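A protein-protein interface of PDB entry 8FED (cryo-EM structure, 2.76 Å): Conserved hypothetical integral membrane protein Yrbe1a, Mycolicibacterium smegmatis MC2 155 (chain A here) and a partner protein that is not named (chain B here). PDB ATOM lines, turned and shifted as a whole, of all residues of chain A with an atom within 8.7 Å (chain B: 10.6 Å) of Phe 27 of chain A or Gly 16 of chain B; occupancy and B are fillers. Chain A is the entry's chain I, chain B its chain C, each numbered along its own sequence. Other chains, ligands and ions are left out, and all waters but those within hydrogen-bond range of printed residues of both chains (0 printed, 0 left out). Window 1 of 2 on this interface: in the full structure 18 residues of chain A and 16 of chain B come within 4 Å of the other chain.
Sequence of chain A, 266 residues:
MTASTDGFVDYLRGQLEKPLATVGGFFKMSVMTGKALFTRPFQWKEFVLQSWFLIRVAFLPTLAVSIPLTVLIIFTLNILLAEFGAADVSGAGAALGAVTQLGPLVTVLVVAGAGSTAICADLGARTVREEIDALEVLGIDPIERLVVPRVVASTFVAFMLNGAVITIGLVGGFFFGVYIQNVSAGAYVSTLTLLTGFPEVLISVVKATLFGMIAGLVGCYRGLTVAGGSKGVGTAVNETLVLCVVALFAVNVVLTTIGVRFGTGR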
ATOM      1  N   PRO A  19     -19.370 -13.749  15.739  1.00  0.00           N
ATOM      2  CA  PRO A  19     -20.243 -12.858  14.953  1.00  0.00           C
ATOM      3  C   PRO A  19     -21.113 -11.960  15.814  1.00  0.00           C
ATOM      4  O   PRO A  19     -21.353 -10.802  15.451  1.00  0.00           O
ATOM      5  CB  PRO A  19     -21.083 -13.833  14.116  1.00  0.00           C
ATOM      6  CG  PRO A  19     -20.273 -15.063  14.043  1.00  0.00           C
ATOM      7  CD  PRO A  19     -19.589 -15.162  15.367  1.00  0.00           C
ATOM      8  N   LEU A  20     -21.583 -12.462  16.959  1.00  0.00           N
ATOM      9  CA  LEU A  20     -22.377 -11.632  17.857  1.00  0.00           C
ATOM     10  C   LEU A  20     -21.543 -10.496  18.434  1.00  0.00           C
ATOM     11  O   LEU A  20     -22.036  -9.375  18.591  1.00  0.00           O
ATOM     12  CB  LEU A  20     -22.971 -12.487  18.974  1.00  0.00           C
ATOM     13  CG  LEU A  20     -24.236 -11.959  19.649  1.00  0.00           C
ATOM     14  CD1 LEU A  20     -25.236 -11.475  18.613  1.00  0.00           C
ATOM     15  CD2 LEU A  20     -24.847 -13.043  20.513  1.00  0.00           C
ATOM     16  N   ALA A  21     -20.276 -10.767  18.752  1.00  0.00           N
ATOM     17  CA  ALA A  21     -19.384  -9.713  19.223  1.00  0.00           C
ATOM     18  C   ALA A  21     -19.135  -8.670  18.141  1.00  0.00           C
ATOM     19  O   ALA A  21     -19.084  -7.469  18.427  1.00  0.00           O
ATOM     20  CB  ALA A  21     -18.066 -10.318  19.701  1.00  0.00           C
ATOM     21  N   THR A  22     -18.965  -9.108  16.890  1.00  0.00           N
ATOM     22  CA  THR A  22     -18.798  -8.148  15.800  1.00  0.00           C
ATOM     23  C   THR A  22     -20.046  -7.288  15.627  1.00  0.00           C
ATOM     24  O   THR A  22     -19.950  -6.074  15.403  1.00  0.00           O
ATOM     25  CB  THR A  22     -18.461  -8.870  14.497  1.00  0.00           C
ATOM     26  OG1 THR A  22     -19.510  -9.789  14.170  1.00  0.00           O
ATOM     27  CG2 THR A  22     -17.147  -9.622  14.628  1.00  0.00           C
ATOM     28  N   VAL A  23     -21.226  -7.905  15.727  1.00  0.00           N
ATOM     29  CA  VAL A  23     -22.478  -7.158  15.641  1.00  0.00           C
ATOM     30  C   VAL A  23     -22.581  -6.157  16.788  1.00  0.00           C
ATOM     31  O   VAL A  23     -23.035  -5.020  16.602  1.00  0.00           O
ATOM     32  CB  VAL A  23     -23.672  -8.130  15.616  1.00  0.00           C
ATOM     33  CG1 VAL A  23     -24.977  -7.391  15.806  1.00  0.00           C
ATOM     34  CG2 VAL A  23     -23.698  -8.898  14.305  1.00  0.00           C
ATOM     35  N   GLY A  24     -22.161  -6.562  17.987  1.00  0.00           N
ATOM     36  CA  GLY A  24     -22.169  -5.644  19.114  1.00  0.00           C
ATOM     37  C   GLY A  24     -21.226  -4.474  18.927  1.00  0.00           C
ATOM     38  O   GLY A  24     -21.549  -3.340  19.288  1.00  0.00           O
ATOM     39  N   GLY A  25     -20.042  -4.737  18.376  1.00  0.00           N
ATOM     40  CA  GLY A  25     -19.132  -3.651  18.054  1.00  0.00           C
ATOM     41  C   GLY A  25     -19.724  -2.688  17.045  1.00  0.00           C
ATOM     42  O   GLY A  25     -19.602  -1.468  17.190  1.00  0.00           O
ATOM     43  N   PHE A  26     -20.385  -3.224  16.015  1.00  0.00           N
ATOM     44  CA  PHE A  26     -21.049  -2.373  15.030  1.00  0.00           C
ATOM     45  C   PHE A  26     -22.131  -1.516  15.674  1.00  0.00           C
ATOM     46  O   PHE A  26     -22.238  -0.317  15.389  1.00  0.00           O
ATOM     47  CB  PHE A  26     -21.641  -3.234  13.913  1.00  0.00           C
ATOM     48  CG  PHE A  26     -22.587  -2.496  13.009  1.00  0.00           C
ATOM     49  CD1 PHE A  26     -22.107  -1.698  11.986  1.00  0.00           C
ATOM     50  CD2 PHE A  26     -23.958  -2.617  13.168  1.00  0.00           C
ATOM     51  CE1 PHE A  26     -22.973  -1.023  11.149  1.00  0.00           C
ATOM     52  CE2 PHE A  26     -24.828  -1.944  12.334  1.00  0.00           C
ATOM     53  CZ  PHE A  26     -24.335  -1.146  11.324  1.00  0.00           C
ATOM     54  N   PHE A  27     -22.951  -2.118  16.539  1.00  0.00           N
ATOM     55  CA  PHE A  27     -24.027  -1.373  17.185  1.00  0.00           C
ATOM     56  C   PHE A  27     -23.486  -0.291  18.108  1.00  0.00           C
ATOM     57  O   PHE A  27     -24.007   0.830  18.130  1.00  0.00           O
ATOM     58  CB  PHE A  27     -24.945  -2.329  17.943  1.00  0.00           C
ATOM     59  CG  PHE A  27     -25.973  -2.989  17.073  1.00  0.00           C
ATOM     60  CD1 PHE A  27     -26.524  -2.312  15.998  1.00  0.00           C
ATOM     61  CD2 PHE A  27     -26.386  -4.284  17.321  1.00  0.00           C
ATOM     62  CE1 PHE A  27     -27.470  -2.912  15.193  1.00  0.00           C
ATOM     63  CE2 PHE A  27     -27.335  -4.888  16.522  1.00  0.00           C
ATOM     64  CZ  PHE A  27     -27.875  -4.202  15.454  1.00  0.00           C
ATOM     65  N   LYS A  28     -22.441  -0.604  18.881  1.00  0.00           N
ATOM     66  CA  LYS A  28     -21.839   0.400  19.752  1.00  0.00           C
ATOM     67  C   LYS A  28     -21.235   1.538  18.940  1.00  0.00           C
ATOM     68  O   LYS A  28     -21.353   2.712  19.313  1.00  0.00           O
ATOM     69  CB  LYS A  28     -20.782  -0.248  20.646  1.00  0.00           C
ATOM     70  CG  LYS A  28     -20.132   0.710  21.626  1.00  0.00           C
ATOM     71  CD  LYS A  28     -19.209  -0.022  22.582  1.00  0.00           C
ATOM     72  CE  LYS A  28     -18.157  -0.814  21.829  1.00  0.00           C
ATOM     73  NZ  LYS A  28     -17.353   0.060  20.933  1.00  0.00           N
ATOM     74  N   MET A  29     -20.587   1.207  17.820  1.00  0.00           N
ATOM     75  CA  MET A  29     -20.029   2.234  16.950  1.00  0.00           C
ATOM     76  C   MET A  29     -21.121   3.132  16.380  1.00  0.00           C
ATOM     77  O   MET A  29     -20.958   4.355  16.316  1.00  0.00           O
ATOM     78  CB  MET A  29     -19.222   1.571  15.836  1.00  0.00           C
ATOM     79  CG  MET A  29     -18.561   2.523  14.872  1.00  0.00           C
ATOM     80  SD  MET A  29     -19.531   2.761  13.381  1.00  0.00           S
ATOM     81  CE  MET A  29     -18.239   3.286  12.275  1.00  0.00           C
ATOM     82  N   SER A  30     -22.244   2.542  15.963  1.00  0.00           N
ATOM     83  CA  SER A  30     -23.347   3.338  15.429  1.00  0.00           C
ATOM     84  C   SER A  30     -23.962   4.229  16.504  1.00  0.00           C
ATOM     85  O   SER A  30     -24.339   5.375  16.227  1.00  0.00           O
ATOM     86  CB  SER A  30     -24.405   2.424  14.816  1.00  0.00           C
ATOM     87  OG  SER A  30     -24.895   1.502  15.771  1.00  0.00           O
ATOM     88  N   VAL A  31     -24.086   3.715  17.730  1.00  0.00           N
ATOM     89  CA  VAL A  31     -24.608   4.523  18.831  1.00  0.00           C
ATOM     90  C   VAL A  31     -23.687   5.704  19.109  1.00  0.00           C
ATOM     91  O   VAL A  31     -24.144   6.835  19.317  1.00  0.00           O
ATOM     92  CB  VAL A  31     -24.813   3.651  20.084  1.00  0.00           C
ATOM     93  CG1 VAL A  31     -25.063   4.518  21.304  1.00  0.00           C
ATOM     94  CG2 VAL A  31     -25.975   2.700  19.874  1.00  0.00           C
ATOM     95  N   MET A  32     -22.373   5.460  19.118  1.00  0.00           N
ATOM     96  CA  MET A  32     -21.424   6.552  19.314  1.00  0.00           C
ATOM     97  C   MET A  32     -21.500   7.561  18.174  1.00  0.00           C
ATOM     98  O   MET A  32     -21.368   8.770  18.397  1.00  0.00           O
ATOM     99  CB  MET A  32     -20.007   5.998  19.456  1.00  0.00           C
ATOM    100  CG  MET A  32     -19.768   5.256  20.762  1.00  0.00           C
ATOM    101  SD  MET A  32     -18.047   4.780  21.012  1.00  0.00           S
ATOM    102  CE  MET A  32     -17.874   3.464  19.811  1.00  0.00           C
ATOM    103  N   THR A  33     -21.712   7.081  16.944  1.00  0.00           N
ATOM    104  CA  THR A  33     -21.881   7.982  15.807  1.00  0.00           C
ATOM    105  C   THR A  33     -23.103   8.874  15.984  1.00  0.00           C
ATOM    106  O   THR A  33     -23.041  10.085  15.736  1.00  0.00           O
ATOM    107  CB  THR A  33     -21.996   7.171  14.516  1.00  0.00           C
ATOM    108  OG1 THR A  33     -20.772   6.466  14.284  1.00  0.00           O
ATOM    109  CG2 THR A  33     -22.286   8.077  13.330  1.00  0.00           C
ATOM    110  N   GLY A  34     -24.224   8.292  16.415  1.00  0.00           N
ATOM    111  CA  GLY A  34     -25.420   9.089  16.648  1.00  0.00           C
ATOM    112  C   GLY A  34     -25.234  10.107  17.757  1.00  0.00           C
ATOM    113  O   GLY A  34     -25.687  11.252  17.649  1.00  0.00           O
ATOM    114  N   ILE A 214     -27.771   2.685   6.671  1.00  0.00           N
ATOM    115  CA  ILE A 214     -27.215   1.378   7.008  1.00  0.00           C
ATOM    116  C   ILE A 214     -25.967   1.091   6.182  1.00  0.00           C
ATOM    117  O   ILE A 214     -24.977   0.558   6.697  1.00  0.00           O
ATOM    118  CB  ILE A 214     -28.281   0.282   6.838  1.00  0.00           C
ATOM    119  CG1 ILE A 214     -29.417   0.486   7.842  1.00  0.00           C
ATOM    120  CG2 ILE A 214     -27.674  -1.096   7.023  1.00  0.00           C
ATOM    121  CD1 ILE A 214     -30.546  -0.505   7.693  1.00  0.00           C
ATOM    122  N   LEU A 217     -23.111   3.137   7.656  1.00  0.00           N
ATOM    123  CA  LEU A 217     -22.664   2.596   8.935  1.00  0.00           C
ATOM    124  C   LEU A 217     -21.848   1.323   8.749  1.00  0.00           C
ATOM    125  O   LEU A 217     -20.790   1.161   9.370  1.00  0.00           O
ATOM    126  CB  LEU A 217     -23.862   2.334   9.846  1.00  0.00           C
ATOM    127  CG  LEU A 217     -24.532   3.562  10.462  1.00  0.00           C
ATOM    128  CD1 LEU A 217     -25.743   3.151  11.279  1.00  0.00           C
ATOM    129  CD2 LEU A 217     -23.542   4.323  11.323  1.00  0.00           C
ATOM    130  N   VAL A 218     -22.318   0.410   7.894  1.00  0.00           N
ATOM    131  CA  VAL A 218     -21.599  -0.841   7.670  1.00  0.00           C
ATOM    132  C   VAL A 218     -20.247  -0.577   7.023  1.00  0.00           C
ATOM    133  O   VAL A 218     -19.228  -1.153   7.429  1.00  0.00           O
ATOM    134  CB  VAL A 218     -22.454  -1.810   6.831  1.00  0.00           C
ATOM    135  CG1 VAL A 218     -21.645  -3.034   6.445  1.00  0.00           C
ATOM    136  CG2 VAL A 218     -23.688  -2.231   7.607  1.00  0.00           C
ATOM    137  N   TYR A 221     -17.896   0.976   9.679  1.00  0.00           N
ATOM    138  CA  TYR A 221     -17.494   0.020  10.707  1.00  0.00           C
ATOM    139  C   TYR A 221     -16.509  -1.004  10.165  1.00  0.00           C
ATOM    140  O   TYR A 221     -15.551  -1.373  10.854  1.00  0.00           O
ATOM    141  CB  TYR A 221     -18.710  -0.686  11.295  1.00  0.00           C
ATOM    142  CG  TYR A 221     -18.332  -1.730  12.319  1.00  0.00           C
ATOM    143  CD1 TYR A 221     -17.802  -1.364  13.547  1.00  0.00           C
ATOM    144  CD2 TYR A 221     -18.495  -3.082  12.054  1.00  0.00           C
ATOM    145  CE1 TYR A 221     -17.450  -2.311  14.484  1.00  0.00           C
ATOM    146  CE2 TYR A 221     -18.146  -4.038  12.986  1.00  0.00           C
ATOM    147  CZ  TYR A 221     -17.624  -3.646  14.199  1.00  0.00           C
ATOM    148  OH  TYR A 221     -17.274  -4.591  15.134  1.00  0.00           O
ATOM    149  N   THR B   3     -11.805   1.320  21.700  1.00  0.00           N
ATOM    150  CA  THR B   3     -13.210   1.321  22.095  1.00  0.00           C
ATOM    151  C   THR B   3     -14.005   0.249  21.360  1.00  0.00           C
ATOM    152  O   THR B   3     -14.831  -0.444  21.966  1.00  0.00           O
ATOM    153  CB  THR B   3     -13.823   2.699  21.848  1.00  0.00           C
ATOM    154  OG1 THR B   3     -13.681   3.044  20.465  1.00  0.00           O
ATOM    155  CG2 THR B   3     -13.127   3.749  22.699  1.00  0.00           C
ATOM    156  N   LEU B   4     -13.781   0.107  20.051  1.00  0.00           N
ATOM    157  CA  LEU B   4     -14.515  -0.889  19.274  1.00  0.00           C
ATOM    158  C   LEU B   4     -14.165  -2.307  19.709  1.00  0.00           C
ATOM    159  O   LEU B   4     -15.046  -3.171  19.792  1.00  0.00           O
ATOM    160  CB  LEU B   4     -14.235  -0.704  17.784  1.00  0.00           C
ATOM    161  CG  LEU B   4     -14.609   0.653  17.185  1.00  0.00           C
ATOM    162  CD1 LEU B   4     -14.410   0.649  15.679  1.00  0.00           C
ATOM    163  CD2 LEU B   4     -16.038   1.017  17.540  1.00  0.00           C
ATOM    164  N   ASP B   8     -16.744  -5.972  25.847  1.00  0.00           N
ATOM    165  CA  ASP B   8     -18.149  -5.832  26.207  1.00  0.00           C
ATOM    166  C   ASP B   8     -19.049  -5.999  24.988  1.00  0.00           C
ATOM    167  O   ASP B   8     -20.205  -5.559  25.014  1.00  0.00           O
ATOM    168  CB  ASP B   8     -18.416  -4.477  26.870  1.00  0.00           C
ATOM    169  CG  ASP B   8     -18.184  -3.310  25.928  1.00  0.00           C
ATOM    170  OD1 ASP B   8     -17.318  -3.426  25.036  1.00  0.00           O
ATOM    171  OD2 ASP B   8     -18.869  -2.278  26.081  1.00  0.00           O
ATOM    172  N   ARG B   9     -18.542  -6.621  23.923  1.00  0.00           N
ATOM    173  CA  ARG B   9     -19.272  -6.676  22.662  1.00  0.00           C
ATOM    174  C   ARG B   9     -20.457  -7.633  22.716  1.00  0.00           C
ATOM    175  O   ARG B   9     -21.410  -7.468  21.950  1.00  0.00           O
ATOM    176  CB  ARG B   9     -18.322  -7.077  21.535  1.00  0.00           C
ATOM    177  CG  ARG B   9     -17.401  -5.967  21.051  1.00  0.00           C
ATOM    178  CD  ARG B   9     -16.440  -6.499  19.998  1.00  0.00           C
ATOM    179  NE  ARG B   9     -15.954  -5.451  19.107  1.00  0.00           N
ATOM    180  CZ  ARG B   9     -15.264  -5.674  17.998  1.00  0.00           C
ATOM    181  NH1 ARG B   9     -14.951  -6.901  17.613  1.00  0.00           N
ATOM    182  NH2 ARG B   9     -14.879  -4.642  17.254  1.00  0.00           N
ATOM    183  N   PHE B  10     -20.419  -8.640  23.592  1.00  0.00           N
ATOM    184  CA  PHE B  10     -21.513  -9.606  23.654  1.00  0.00           C
ATOM    185  C   PHE B  10     -22.789  -8.963  24.191  1.00  0.00           C
ATOM    186  O   PHE B  10     -23.878  -9.148  23.629  1.00  0.00           O
ATOM    187  CB  PHE B  10     -21.103 -10.802  24.514  1.00  0.00           C
ATOM    188  CG  PHE B  10     -22.119 -11.909  24.539  1.00  0.00           C
ATOM    189  CD1 PHE B  10     -22.144 -12.864  23.537  1.00  0.00           C
ATOM    190  CD2 PHE B  10     -23.042 -12.001  25.568  1.00  0.00           C
ATOM    191  CE1 PHE B  10     -23.073 -13.886  23.557  1.00  0.00           C
ATOM    192  CE2 PHE B  10     -23.974 -13.021  25.593  1.00  0.00           C
ATOM    193  CZ  PHE B  10     -23.989 -13.964  24.586  1.00  0.00           C
ATOM    194  N   ARG B  11     -22.673  -8.213  25.289  1.00  0.00           N
ATOM    195  CA  ARG B  11     -23.829  -7.519  25.845  1.00  0.00           C
ATOM    196  C   ARG B  11     -24.358  -6.476  24.870  1.00  0.00           C
ATOM    197  O   ARG B  11     -25.577  -6.313  24.720  1.00  0.00           O
ATOM    198  CB  ARG B  11     -23.455  -6.878  27.181  1.00  0.00           C
ATOM    199  CG  ARG B  11     -24.579  -6.117  27.855  1.00  0.00           C
ATOM    200  CD  ARG B  11     -24.241  -5.810  29.303  1.00  0.00           C
ATOM    201  NE  ARG B  11     -22.984  -5.084  29.432  1.00  0.00           N
ATOM    202  CZ  ARG B  11     -22.397  -4.803  30.588  1.00  0.00           C
ATOM    203  NH1 ARG B  11     -22.927  -5.177  31.741  1.00  0.00           N
ATOM    204  NH2 ARG B  11     -21.250  -4.130  30.587  1.00  0.00           N
ATOM    205  N   LYS B  12     -23.452  -5.760  24.199  1.00  0.00           N
ATOM    206  CA  LYS B  12     -23.863  -4.795  23.186  1.00  0.00           C
ATOM    207  C   LYS B  12     -24.614  -5.477  22.052  1.00  0.00           C
ATOM    208  O   LYS B  12     -25.621  -4.953  21.565  1.00  0.00           O
ATOM    209  CB  LYS B  12     -22.641  -4.049  22.648  1.00  0.00           C
ATOM    210  CG  LYS B  12     -22.599  -2.577  23.021  1.00  0.00           C
ATOM    211  CD  LYS B  12     -22.557  -2.390  24.528  1.00  0.00           C
ATOM    212  CE  LYS B  12     -22.552  -0.917  24.898  1.00  0.00           C
ATOM    213  NZ  LYS B  12     -22.485  -0.715  26.370  1.00  0.00           N
ATOM    214  N   GLY B  13     -24.141  -6.648  21.619  1.00  0.00           N
ATOM    215  CA  GLY B  13     -24.827  -7.372  20.561  1.00  0.00           C
ATOM    216  C   GLY B  13     -26.211  -7.831  20.969  1.00  0.00           C
ATOM    217  O   GLY B  13     -27.166  -7.704  20.201  1.00  0.00           O
ATOM    218  N   LEU B  14     -26.333  -8.375  22.185  1.00  0.00           N
ATOM    219  CA  LEU B  14     -27.643  -8.780  22.689  1.00  0.00           C
ATOM    220  C   LEU B  14     -28.602  -7.597  22.730  1.00  0.00           C
ATOM    221  O   LEU B  14     -29.726  -7.669  22.213  1.00  0.00           O
ATOM    222  CB  LEU B  14     -27.504  -9.403  24.077  1.00  0.00           C
ATOM    223  CG  LEU B  14     -27.677 -10.919  24.173  1.00  0.00           C
ATOM    224  CD1 LEU B  14     -26.574 -11.629  23.416  1.00  0.00           C
ATOM    225  CD2 LEU B  14     -27.705 -11.361  25.627  1.00  0.00           C
ATOM    226  N   MET B  15     -28.163  -6.487  23.334  1.00  0.00           N
ATOM    227  CA  MET B  15     -29.023  -5.317  23.455  1.00  0.00           C
ATOM    228  C   MET B  15     -29.413  -4.777  22.086  1.00  0.00           C
ATOM    229  O   MET B  15     -30.583  -4.459  21.846  1.00  0.00           O
ATOM    230  CB  MET B  15     -28.323  -4.240  24.284  1.00  0.00           C
ATOM    231  CG  MET B  15     -29.132  -2.973  24.480  1.00  0.00           C
ATOM    232  SD  MET B  15     -28.508  -1.974  25.843  1.00  0.00           S
ATOM    233  CE  MET B  15     -26.781  -1.828  25.395  1.00  0.00           C
ATOM    234  N   GLY B  16     -28.451  -4.696  21.165  1.00  0.00           N
ATOM    235  CA  GLY B  16     -28.743  -4.161  19.848  1.00  0.00           C
ATOM    236  C   GLY B  16     -29.686  -5.034  19.044  1.00  0.00           C
ATOM    237  O   GLY B  16     -30.588  -4.523  18.376  1.00  0.00           O
ATOM    238  N   VAL B  17     -29.493  -6.355  19.083  1.00  0.00           N
ATOM    239  CA  VAL B  17     -30.367  -7.230  18.309  1.00  0.00           C
ATOM    240  C   VAL B  17     -31.777  -7.220  18.893  1.00  0.00           C
ATOM    241  O   VAL B  17     -32.767  -7.240  18.148  1.00  0.00           O
ATOM    242  CB  VAL B  17     -29.779  -8.653  18.199  1.00  0.00           C
ATOM    243  CG1 VAL B  17     -29.811  -9.403  19.524  1.00  0.00           C
ATOM    244  CG2 VAL B  17     -30.500  -9.442  17.115  1.00  0.00           C
ATOM    245  N   ILE B  18     -31.899  -7.151  20.225  1.00  0.00           N
ATOM    246  CA  ILE B  18     -33.225  -7.050  20.830  1.00  0.00           C
ATOM    247  C   ILE B  18     -33.893  -5.738  20.434  1.00  0.00           C
ATOM    248  O   ILE B  18     -35.087  -5.709  20.106  1.00  0.00           O
ATOM    249  CB  ILE B  18     -33.131  -7.211  22.359  1.00  0.00           C
ATOM    250  CG1 ILE B  18     -32.734  -8.645  22.713  1.00  0.00           C
ATOM    251  CG2 ILE B  18     -34.450  -6.852  23.024  1.00  0.00           C
ATOM    252  CD1 ILE B  18     -32.663  -8.913  24.199  1.00  0.00           C
ATOM    253  N   VAL B  19     -33.133  -4.639  20.433  1.00  0.00           N
ATOM    254  CA  VAL B  19     -33.694  -3.342  20.062  1.00  0.00           C
ATOM    255  C   VAL B  19     -34.145  -3.341  18.604  1.00  0.00           C
ATOM    256  O   VAL B  19     -35.219  -2.827  18.275  1.00  0.00           O
ATOM    257  CB  VAL B  19     -32.678  -2.219  20.349  1.00  0.00           C
ATOM    258  CG1 VAL B  19     -33.073  -0.936  19.636  1.00  0.00           C
ATOM    259  CG2 VAL B  19     -32.582  -1.972  21.843  1.00  0.00           C
ATOM    260  N   VAL B  20     -33.337  -3.918  17.711  1.00  0.00           N
ATOM    261  CA  VAL B  20     -33.699  -3.948  16.295  1.00  0.00           C
ATOM    262  C   VAL B  20     -34.934  -4.813  16.070  1.00  0.00           C
ATOM    263  O   VAL B  20     -35.831  -4.446  15.298  1.00  0.00           O
ATOM    264  CB  VAL B  20     -32.505  -4.417  15.444  1.00  0.00           C
ATOM    265  CG1 VAL B  20     -32.932  -4.650  14.005  1.00  0.00           C
ATOM    266  CG2 VAL B  20     -31.396  -3.385  15.488  1.00  0.00           C
ATOM    267  N   ALA B  21     -35.008  -5.968  16.739  1.00  0.00           N
ATOM    268  CA  ALA B  21     -36.198  -6.807  16.627  1.00  0.00           C
ATOM    269  C   ALA B  21     -37.435  -6.077  17.137  1.00  0.00           C
ATOM    270  O   ALA B  21     -38.508  -6.152  16.525  1.00  0.00           O
ATOM    271  CB  ALA B  21     -35.992  -8.116  17.387  1.00  0.00           C
ATOM    272  N   LEU B  22     -37.299  -5.358  18.256  1.00  0.00           N
ATOM    273  CA  LEU B  22     -38.418  -4.587  18.789  1.00  0.00           C
ATOM    274  C   LEU B  22     -38.856  -3.498  17.818  1.00  0.00           C
ATOM    275  O   LEU B  22     -40.056  -3.284  17.618  1.00  0.00           O
ATOM    276  CB  LEU B  22     -38.036  -3.976  20.137  1.00  0.00           C
ATOM    277  CG  LEU B  22     -38.442  -4.708  21.417  1.00  0.00           C
ATOM    278  CD1 LEU B  22     -38.109  -6.189  21.354  1.00  0.00           C
ATOM    279  CD2 LEU B  22     -37.760  -4.060  22.612  1.00  0.00           C
ATOM    280  N   ILE B  23     -37.896  -2.796  17.211  1.00  0.00           N
ATOM    281  CA  ILE B  23     -38.227  -1.732  16.265  1.00  0.00           C
ATOM    282  C   ILE B  23     -38.957  -2.301  15.055  1.00  0.00           C
ATOM    283  O   ILE B  23     -39.947  -1.728  14.583  1.00  0.00           O
ATOM    284  CB  ILE B  23     -36.954  -0.965  15.856  1.00  0.00           C
ATOM    285  CG1 ILE B  23     -36.438  -0.129  17.029  1.00  0.00           C
ATOM    286  CG2 ILE B  23     -37.217  -0.077  14.651  1.00  0.00           C
ATOM    287  CD1 ILE B  23     -35.178   0.643  16.718  1.00  0.00           C
ATOM    288  N   ILE B  24     -38.483  -3.438  14.539  1.00  0.00           N
ATOM    289  CA  ILE B  24     -39.140  -4.070  13.397  1.00  0.00           C
ATOM    290  C   ILE B  24     -40.557  -4.495  13.765  1.00  0.00           C
ATOM    291  O   ILE B  24     -41.503  -4.290  12.994  1.00  0.00           O
ATOM    292  CB  ILE B  24     -38.298  -5.255  12.887  1.00  0.00           C
ATOM    293  CG1 ILE B  24     -36.977  -4.754  12.301  1.00  0.00           C
ATOM    294  CG2 ILE B  24     -39.069  -6.064  11.857  1.00  0.00           C
ATOM    295  CD1 ILE B  24     -36.081  -5.853  11.781  1.00  0.00           C
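NZ of Lys 28 of chain A sits at hydrogen-bond distance from O of Thr 3 of chain B (2.8 Å). The guanidinium group (NH2) of Arg 9 of chain B sits at hydrogen-bond distance from the side-chain hydroxyl (OH) of Tyr 221 of chain A (3.2 Å).
The backbone carbonyl oxygen (O) of Leu 4 of chain B sits at hydrogen-bond distance from the guanidinium group (NE) of Arg 9 of chain B (2.5 Å). The side-chain carboxylate (OD2) of Asp 8 of chain B lies within salt-bridge range of the side-chain amino group (NZ) of Lys 12 of chain B (3.9 Å). OH of Tyr 221 of chain A lies within hydrogen-bond range of O of Thr 22 of chain A (3.1 Å). The side-chain hydroxyl (OG) of Ser 30 of chain A is in hydrogen-bond range of the backbone carbonyl oxygen (O) of Phe 27 of chain A (2.6 Å). OG1 of Thr 33 of chain A sits at hydrogen-bond distance from O of Met 29 of chain A (2.9 Å).
Among the printed residues, merely in contact across the chains: Leu 20 of chain A with Arg 9 of chain B (3.9 Å), Leu 20 of chain A with Phe 10 of chain B (3.6 Å), Leu 20 of chain A with Gly 13 of chain B (3.96 Å), Leu 20 of chain A with Leu 14 of chain B (3.7 Å), Ala 21 of chain A with Arg 9 of chain B (3.2 Å), Gly 24 of chain A with Arg 9 of chain B (3.5 Å), Gly 24 of chain A with Lys 12 of chain B (3.6 Å), Gly 24 of chain A with Gly 13 of chain B (3.3 Å), Gly 25 of chain A with Arg 9 of chain B (3.8 Å), Phe 27 of chain A with Gly 16 of chain B (3.5 Å), Phe 27 of chain A with Val 17 of chain B (3.7 Å), Phe 27 of chain A with Val 20 of chain B (3.6 Å), Lys 28 of chain A with Leu 4 of chain B (3.4 Å), Lys 28 of chain A with Lys 12 of chain B (3.8 Å), Met 29 of chain A with Leu 4 of chain B (3.7 Å) and Met 32 of chain A with Leu 4 of chain B (3.8 Å).
Printed residues of chain B within 4 Å of Leu 20 of chain A: Arg 9, Phe 10, Gly 13 and Leu 14. Gly 24 of chain A touches just these residues of chain B: Arg 9 (3.5 Å), Lys 12 (3.6 Å) and Gly 13 (3.3 Å). Gly 25 of chain A touches just one residue of chain B: Arg 9. No residue of chain B comes within 4 Å of Phe 26 of chain A. Phe 27 of chain A touches just these residues of chain B: Gly 16, Val 17 and Val 20. Of the printed residues of chain B, Lys 28 of chain A touches Thr 3, Leu 4 and Lys 12. No residue of chain B comes within 4 Å of Val 31 of chain A. Printed residues of chain A within 4 Å of Phe 10 of chain B: Leu 20 (3.6 Å). Gly 16 of chain B touches one residue of chain A. The nearest residue of chain B that does not touch Phe 27 of chain A is Lys 12 of chain B (4.4 Å). The nearest printed residue of chain A that does not touch Leu 4 of chain B is Gly 25 of chain A (4.4 Å).
Hydrophobic or aromatic side chains of chain B that line the printed part of chain A: Leu 4, Phe 10, Leu 14 and Val 20. Of the 20 printed residues of chain A, 9 touch a printed residue of chain B. Hydrophobic or aromatic side chains of chain A within 4 Å of the printed part of chain B: Leu 20, Ala 21, Phe 27, Met 29, Met 32 and Tyr 221. Along chain A the printed residues that touch a printed residue of chain B span positions 20 to 221. Among the printed residues, 18 pairs touch across the chains. Among the printed residues, no Asp or Glu carboxylate lies within 4 Å of a Lys or Arg side-chain nitrogen of the other chain.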
